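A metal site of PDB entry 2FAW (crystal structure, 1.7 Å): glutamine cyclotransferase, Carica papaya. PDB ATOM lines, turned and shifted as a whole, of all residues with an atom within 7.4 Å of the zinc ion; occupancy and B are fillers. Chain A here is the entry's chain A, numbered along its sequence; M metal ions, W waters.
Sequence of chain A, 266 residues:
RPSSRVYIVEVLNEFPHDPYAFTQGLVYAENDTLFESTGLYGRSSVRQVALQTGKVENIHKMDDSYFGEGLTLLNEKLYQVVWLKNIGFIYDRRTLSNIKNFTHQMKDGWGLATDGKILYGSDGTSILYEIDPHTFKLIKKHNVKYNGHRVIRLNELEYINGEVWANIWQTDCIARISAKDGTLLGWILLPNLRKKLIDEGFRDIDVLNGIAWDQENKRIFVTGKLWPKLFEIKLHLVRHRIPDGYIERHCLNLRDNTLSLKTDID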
ATOM      1  N   GLN A  24      21.240  17.729  26.112  1.00  0.00           N
ATOM      2  CA  GLN A  24      22.343  17.217  25.339  1.00  0.00           C
ATOM      3  C   GLN A  24      22.881  18.319  24.489  1.00  0.00           C
ATOM      4  O   GLN A  24      23.912  18.170  23.897  1.00  0.00           O
ATOM      5  CB  GLN A  24      21.891  16.088  24.459  1.00  0.00           C
ATOM      6  CG  GLN A  24      21.438  14.873  25.238  1.00  0.00           C
ATOM      7  CD  GLN A  24      22.531  14.001  25.802  1.00  0.00           C
ATOM      8  OE1 GLN A  24      22.231  12.900  26.256  1.00  0.00           O
ATOM      9  NE2 GLN A  24      23.780  14.483  25.805  1.00  0.00           N
ATOM     10  N   GLY A  25      22.163  19.422  24.438  1.00  0.00           N
ATOM     11  CA  GLY A  25      22.642  20.502  23.621  1.00  0.00           C
ATOM     12  C   GLY A  25      22.158  21.728  24.297  1.00  0.00           C
ATOM     13  O   GLY A  25      21.004  21.800  24.679  1.00  0.00           O
ATOM     14  N   LEU A  26      23.046  22.685  24.430  1.00  0.00           N
ATOM     15  CA  LEU A  26      22.641  23.884  25.071  1.00  0.00           C
ATOM     16  C   LEU A  26      23.304  25.009  24.365  1.00  0.00           C
ATOM     17  O   LEU A  26      24.490  24.990  24.102  1.00  0.00           O
ATOM     18  CB  LEU A  26      23.040  23.869  26.548  1.00  0.00           C
ATOM     19  CG  LEU A  26      22.376  25.001  27.310  1.00  0.00           C
ATOM     20  CD1 LEU A  26      20.880  24.769  27.447  1.00  0.00           C
ATOM     21  CD2 LEU A  26      23.022  25.095  28.677  1.00  0.00           C
ATOM     22  N   VAL A  27      22.478  25.984  24.067  1.00  0.00           N
ATOM     23  CA  VAL A  27      22.878  27.081  23.243  1.00  0.00           C
ATOM     24  C   VAL A  27      22.359  28.286  23.924  1.00  0.00           C
ATOM     25  O   VAL A  27      21.264  28.307  24.452  1.00  0.00           O
ATOM     26  CB  VAL A  27      22.183  26.962  21.911  1.00  0.00           C
ATOM     27  CG1 VAL A  27      22.221  28.249  21.123  1.00  0.00           C
ATOM     28  CG2 VAL A  27      22.810  25.843  21.137  1.00  0.00           C
ATOM     29  N   TYR A  28      23.172  29.324  23.924  1.00  0.00           N
ATOM     30  CA  TYR A  28      22.648  30.591  24.311  1.00  0.00           C
ATOM     31  C   TYR A  28      22.529  31.373  23.015  1.00  0.00           C
ATOM     32  O   TYR A  28      23.489  31.494  22.248  1.00  0.00           O
ATOM     33  CB  TYR A  28      23.576  31.278  25.268  1.00  0.00           C
ATOM     34  CG  TYR A  28      23.028  32.607  25.616  1.00  0.00           C
ATOM     35  CD1 TYR A  28      22.250  32.762  26.753  1.00  0.00           C
ATOM     36  CD2 TYR A  28      23.282  33.695  24.805  1.00  0.00           C
ATOM     37  CE1 TYR A  28      21.733  33.990  27.084  1.00  0.00           C
ATOM     38  CE2 TYR A  28      22.765  34.924  25.136  1.00  0.00           C
ATOM     39  CZ  TYR A  28      21.995  35.060  26.264  1.00  0.00           C
ATOM     40  OH  TYR A  28      21.471  36.265  26.616  1.00  0.00           O
ATOM     41  N   PHE A  35      18.728  27.747  23.558  1.00  0.00           N
ATOM     42  CA  PHE A  35      18.161  26.670  22.837  1.00  0.00           C
ATOM     43  C   PHE A  35      18.719  25.468  23.443  1.00  0.00           C
ATOM     44  O   PHE A  35      19.847  25.453  23.908  1.00  0.00           O
ATOM     45  CB  PHE A  35      18.474  26.767  21.387  1.00  0.00           C
ATOM     46  CG  PHE A  35      17.684  27.816  20.705  1.00  0.00           C
ATOM     47  CD1 PHE A  35      16.390  27.545  20.288  1.00  0.00           C
ATOM     48  CD2 PHE A  35      18.210  29.074  20.516  1.00  0.00           C
ATOM     49  CE1 PHE A  35      15.642  28.521  19.656  1.00  0.00           C
ATOM     50  CE2 PHE A  35      17.465  30.067  19.894  1.00  0.00           C
ATOM     51  CZ  PHE A  35      16.180  29.786  19.472  1.00  0.00           C
ATOM     52  N   GLY A  70      23.804  17.099  20.709  1.00  0.00           N
ATOM     53  CA  GLY A  70      24.352  18.435  20.697  1.00  0.00           C
ATOM     54  C   GLY A  70      23.588  19.387  19.836  1.00  0.00           C
ATOM     55  O   GLY A  70      22.894  19.037  18.886  1.00  0.00           O
ATOM     56  N   LEU A  71      23.698  20.636  20.201  1.00  0.00           N
ATOM     57  CA  LEU A  71      22.926  21.630  19.526  1.00  0.00           C
ATOM     58  C   LEU A  71      23.794  22.827  19.523  1.00  0.00           C
ATOM     59  O   LEU A  71      24.418  23.160  20.520  1.00  0.00           O
ATOM     60  CB  LEU A  71      21.685  21.934  20.328  1.00  0.00           C
ATOM     61  CG  LEU A  71      20.758  22.911  19.624  1.00  0.00           C
ATOM     62  CD1 LEU A  71      20.036  22.171  18.526  1.00  0.00           C
ATOM     63  CD2 LEU A  71      19.788  23.472  20.651  1.00  0.00           C
ATOM     64  N   THR A  72      23.810  23.498  18.413  1.00  0.00           N
ATOM     65  CA  THR A  72      24.436  24.770  18.427  1.00  0.00           C
ATOM     66  C   THR A  72      23.669  25.637  17.493  1.00  0.00           C
ATOM     67  O   THR A  72      22.853  25.168  16.731  1.00  0.00           O
ATOM     68  CB  THR A  72      25.903  24.637  18.062  1.00  0.00           C
ATOM     69  OG1 THR A  72      26.529  25.916  18.221  1.00  0.00           O
ATOM     70  CG2 THR A  72      26.109  24.271  16.606  1.00  0.00           C
ATOM     71  N   GLY A 111      28.237  16.359  21.005  1.00  0.00           N
ATOM     72  CA  GLY A 111      28.078  17.777  21.202  1.00  0.00           C
ATOM     73  C   GLY A 111      28.300  18.533  19.936  1.00  0.00           C
ATOM     74  O   GLY A 111      28.914  18.070  18.999  1.00  0.00           O
ATOM     75  N   LEU A 112      27.795  19.743  19.944  1.00  0.00           N
ATOM     76  CA  LEU A 112      28.015  20.655  18.849  1.00  0.00           C
ATOM     77  C   LEU A 112      28.260  21.992  19.421  1.00  0.00           C
ATOM     78  O   LEU A 112      27.700  22.360  20.443  1.00  0.00           O
ATOM     79  CB  LEU A 112      26.796  20.762  17.985  1.00  0.00           C
ATOM     80  CG  LEU A 112      26.549  19.576  17.067  1.00  0.00           C
ATOM     81  CD1 LEU A 112      25.271  19.879  16.303  1.00  0.00           C
ATOM     82  CD2 LEU A 112      27.721  19.371  16.121  1.00  0.00           C
ATOM     83  N   ALA A 113      29.095  22.724  18.734  1.00  0.00           N
ATOM     84  CA  ALA A 113      29.283  24.098  19.104  1.00  0.00           C
ATOM     85  C   ALA A 113      29.657  24.750  17.833  1.00  0.00           C
ATOM     86  O   ALA A 113      29.723  24.124  16.785  1.00  0.00           O
ATOM     87  CB  ALA A 113      30.379  24.247  20.126  1.00  0.00           C
ATOM     88  N   THR A 114      29.850  26.041  17.911  1.00  0.00           N
ATOM     89  CA  THR A 114      30.233  26.709  16.710  1.00  0.00           C
ATOM     90  C   THR A 114      30.996  27.916  17.124  1.00  0.00           C
ATOM     91  O   THR A 114      30.746  28.493  18.166  1.00  0.00           O
ATOM     92  CB  THR A 114      29.018  27.107  15.908  1.00  0.00           C
ATOM     93  OG1 THR A 114      29.453  27.793  14.740  1.00  0.00           O
ATOM     94  CG2 THR A 114      28.189  28.132  16.657  1.00  0.00           C
ATOM     95  N   GLU A 156      28.578  17.777  25.506  1.00  0.00           N
ATOM     96  CA  GLU A 156      28.027  19.043  25.103  1.00  0.00           C
ATOM     97  C   GLU A 156      29.164  20.004  24.949  1.00  0.00           C
ATOM     98  O   GLU A 156      30.100  20.038  25.754  1.00  0.00           O
ATOM     99  CB  GLU A 156      27.012  19.574  26.092  1.00  0.00           C
ATOM    100  CG  GLU A 156      25.855  20.290  25.414  1.00  0.00           C
ATOM    101  CD  GLU A 156      26.148  21.738  25.052  1.00  0.00           C
ATOM    102  OE1 GLU A 156      25.667  22.166  24.007  1.00  0.00           O
ATOM    103  OE2 GLU A 156      26.852  22.439  25.773  1.00  0.00           O
ATOM    104  N   LEU A 157      29.069  20.811  23.917  1.00  0.00           N
ATOM    105  CA  LEU A 157      30.152  21.694  23.613  1.00  0.00           C
ATOM    106  C   LEU A 157      29.639  23.073  23.657  1.00  0.00           C
ATOM    107  O   LEU A 157      28.477  23.321  23.459  1.00  0.00           O
ATOM    108  CB  LEU A 157      30.658  21.457  22.198  1.00  0.00           C
ATOM    109  CG  LEU A 157      31.148  20.062  21.894  1.00  0.00           C
ATOM    110  CD1 LEU A 157      31.680  20.040  20.467  1.00  0.00           C
ATOM    111  CD2 LEU A 157      32.216  19.682  22.899  1.00  0.00           C
ATOM    112  N   GLU A 158      30.561  23.984  23.876  1.00  0.00           N
ATOM    113  CA  GLU A 158      30.233  25.340  23.733  1.00  0.00           C
ATOM    114  C   GLU A 158      31.462  26.009  23.335  1.00  0.00           C
ATOM    115  O   GLU A 158      32.474  25.853  23.966  1.00  0.00           O
ATOM    116  CB  GLU A 158      29.752  25.906  25.049  1.00  0.00           C
ATOM    117  CG  GLU A 158      29.164  27.284  24.879  1.00  0.00           C
ATOM    118  CD  GLU A 158      27.902  27.300  24.059  1.00  0.00           C
ATOM    119  OE1 GLU A 158      27.413  26.252  23.580  1.00  0.00           O
ATOM    120  OE2 GLU A 158      27.381  28.402  23.860  1.00  0.00           O
ATOM    121  N   TYR A 159      31.343  26.798  22.301  1.00  0.00           N
ATOM    122  CA  TYR A 159      32.464  27.577  21.886  1.00  0.00           C
ATOM    123  C   TYR A 159      32.412  28.849  22.665  1.00  0.00           C
ATOM    124  O   TYR A 159      31.416  29.567  22.641  1.00  0.00           O
ATOM    125  CB  TYR A 159      32.322  27.858  20.450  1.00  0.00           C
ATOM    126  CG  TYR A 159      33.392  28.751  19.939  1.00  0.00           C
ATOM    127  CD1 TYR A 159      34.580  28.229  19.493  1.00  0.00           C
ATOM    128  CD2 TYR A 159      33.190  30.113  19.907  1.00  0.00           C
ATOM    129  CE1 TYR A 159      35.539  29.038  18.993  1.00  0.00           C
ATOM    130  CE2 TYR A 159      34.133  30.941  19.402  1.00  0.00           C
ATOM    131  CZ  TYR A 159      35.288  30.408  18.944  1.00  0.00           C
ATOM    132  OH  TYR A 159      36.214  31.244  18.429  1.00  0.00           O
ATOM    133  N   TRP A 165      34.459  24.409  24.944  1.00  0.00           N
ATOM    134  CA  TRP A 165      34.339  23.797  26.218  1.00  0.00           C
ATOM    135  C   TRP A 165      33.486  22.629  25.996  1.00  0.00           C
ATOM    136  O   TRP A 165      32.511  22.680  25.254  1.00  0.00           O
ATOM    137  CB  TRP A 165      33.635  24.713  27.152  1.00  0.00           C
ATOM    138  CG  TRP A 165      34.469  25.846  27.515  1.00  0.00           C
ATOM    139  CD1 TRP A 165      35.588  26.286  26.882  1.00  0.00           C
ATOM    140  CD2 TRP A 165      34.220  26.728  28.580  1.00  0.00           C
ATOM    141  NE1 TRP A 165      36.071  27.411  27.508  1.00  0.00           N
ATOM    142  CE2 TRP A 165      35.247  27.705  28.565  1.00  0.00           C
ATOM    143  CE3 TRP A 165      33.241  26.794  29.567  1.00  0.00           C
ATOM    144  CZ2 TRP A 165      35.306  28.736  29.496  1.00  0.00           C
ATOM    145  CZ3 TRP A 165      33.305  27.801  30.498  1.00  0.00           C
ATOM    146  CH2 TRP A 165      34.331  28.763  30.450  1.00  0.00           C
ATOM    147  N   ASN A 167      31.608  19.509  28.016  1.00  0.00           N
ATOM    148  CA  ASN A 167      31.338  18.645  29.103  1.00  0.00           C
ATOM    149  C   ASN A 167      32.042  17.359  28.836  1.00  0.00           C
ATOM    150  O   ASN A 167      32.143  16.915  27.712  1.00  0.00           O
ATOM    151  CB  ASN A 167      29.872  18.345  29.208  1.00  0.00           C
ATOM    152  CG  ASN A 167      29.126  19.512  29.681  1.00  0.00           C
ATOM    153  OD1 ASN A 167      28.492  20.197  28.915  1.00  0.00           O
ATOM    154  ND2 ASN A 167      29.196  19.766  30.976  1.00  0.00           N
ATOM    155  N   GLY A 210      25.843  20.528  29.189  1.00  0.00           N
ATOM    156  CA  GLY A 210      25.103  21.636  28.669  1.00  0.00           C
ATOM    157  C   GLY A 210      25.830  22.833  29.129  1.00  0.00           C
ATOM    158  O   GLY A 210      25.907  23.168  30.309  1.00  0.00           O
ATOM    159  N   ILE A 211      26.386  23.489  28.155  1.00  0.00           N
ATOM    160  CA  ILE A 211      27.149  24.677  28.406  1.00  0.00           C
ATOM    161  C   ILE A 211      26.663  25.619  27.373  1.00  0.00           C
ATOM    162  O   ILE A 211      26.584  25.279  26.202  1.00  0.00           O
ATOM    163  CB  ILE A 211      28.629  24.451  28.154  1.00  0.00           C
ATOM    164  CG1 ILE A 211      29.181  23.317  29.020  1.00  0.00           C
ATOM    165  CG2 ILE A 211      29.381  25.748  28.443  1.00  0.00           C
ATOM    166  CD1 ILE A 211      30.466  22.767  28.437  1.00  0.00           C
ATOM    167  N   ALA A 212      26.350  26.830  27.795  1.00  0.00           N
ATOM    168  CA  ALA A 212      25.895  27.805  26.834  1.00  0.00           C
ATOM    169  C   ALA A 212      26.591  29.058  27.191  1.00  0.00           C
ATOM    170  O   ALA A 212      26.748  29.378  28.355  1.00  0.00           O
ATOM    171  CB  ALA A 212      24.417  27.972  26.912  1.00  0.00           C
ATOM    172  N   TRP A 213      27.036  29.750  26.168  1.00  0.00           N
ATOM    173  CA  TRP A 213      27.808  30.917  26.374  1.00  0.00           C
ATOM    174  C   TRP A 213      27.079  32.054  25.802  1.00  0.00           C
ATOM    175  O   TRP A 213      26.673  32.060  24.635  1.00  0.00           O
ATOM    176  CB  TRP A 213      29.125  30.760  25.660  1.00  0.00           C
ATOM    177  CG  TRP A 213      29.905  31.980  25.524  1.00  0.00           C
ATOM    178  CD1 TRP A 213      30.311  32.534  24.367  1.00  0.00           C
ATOM    179  CD2 TRP A 213      30.446  32.766  26.576  1.00  0.00           C
ATOM    180  NE1 TRP A 213      31.080  33.653  24.615  1.00  0.00           N
ATOM    181  CE2 TRP A 213      31.169  33.821  25.970  1.00  0.00           C
ATOM    182  CE3 TRP A 213      30.393  32.716  27.977  1.00  0.00           C
ATOM    183  CZ2 TRP A 213      31.837  34.794  26.699  1.00  0.00           C
ATOM    184  CZ3 TRP A 213      31.040  33.688  28.713  1.00  0.00           C
ATOM    185  CH2 TRP A 213      31.780  34.715  28.071  1.00  0.00           C
ATOM    186  N   PHE A 221      26.587  29.454  31.035  1.00  0.00           N
ATOM    187  CA  PHE A 221      25.508  28.752  31.643  1.00  0.00           C
ATOM    188  C   PHE A 221      25.814  27.327  31.496  1.00  0.00           C
ATOM    189  O   PHE A 221      26.248  26.887  30.452  1.00  0.00           O
ATOM    190  CB  PHE A 221      24.231  29.025  30.909  1.00  0.00           C
ATOM    191  CG  PHE A 221      23.855  30.429  30.971  1.00  0.00           C
ATOM    192  CD1 PHE A 221      23.430  30.977  32.184  1.00  0.00           C
ATOM    193  CD2 PHE A 221      23.949  31.222  29.853  1.00  0.00           C
ATOM    194  CE1 PHE A 221      23.078  32.303  32.253  1.00  0.00           C
ATOM    195  CE2 PHE A 221      23.588  32.557  29.927  1.00  0.00           C
ATOM    196  CZ  PHE A 221      23.149  33.078  31.132  1.00  0.00           C
HETATM  197 ZN    ZN M   1      26.561  24.294  24.192  1.00  0.00          ZN
HETATM  198  O   HOH W   1      26.328  24.064  21.929  1.00  0.00           O
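OE2 of Glu 158 is in hydrogen-bond range of N of Trp 213, at 2.7 Å.
O of Glu 158 lies within hydrogen-bond range of N of Trp 165 (2.6 Å).
The backbone NH of Asn 167 lies within hydrogen-bond range of the backbone carbonyl oxygen of Glu 156, 2.8 Å away.
O of Leu 26 binds the zinc ion.
The zinc ion is bound by OE1 of Glu 158, at 2.2 Å.
O of Ile 211 is bound to the zinc ion (2.2 Å).
The zinc ion is bound by the backbone carbonyl oxygen (O) of Leu 157 (2.3 Å).
Water W1 binds the zinc ion, at 2.3 Å.
The zinc ion is bound by OE1 of Glu 156 (2.3 Å).
OE2 of Glu 156 is bound to the zinc ion (2.5 Å).
The zinc ion has seven donor atoms within binding distance.
Water W1 lies within hydrogen-bond range of O of Leu 71 (2.5 Å) and O of Leu 112 (2.6 Å).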
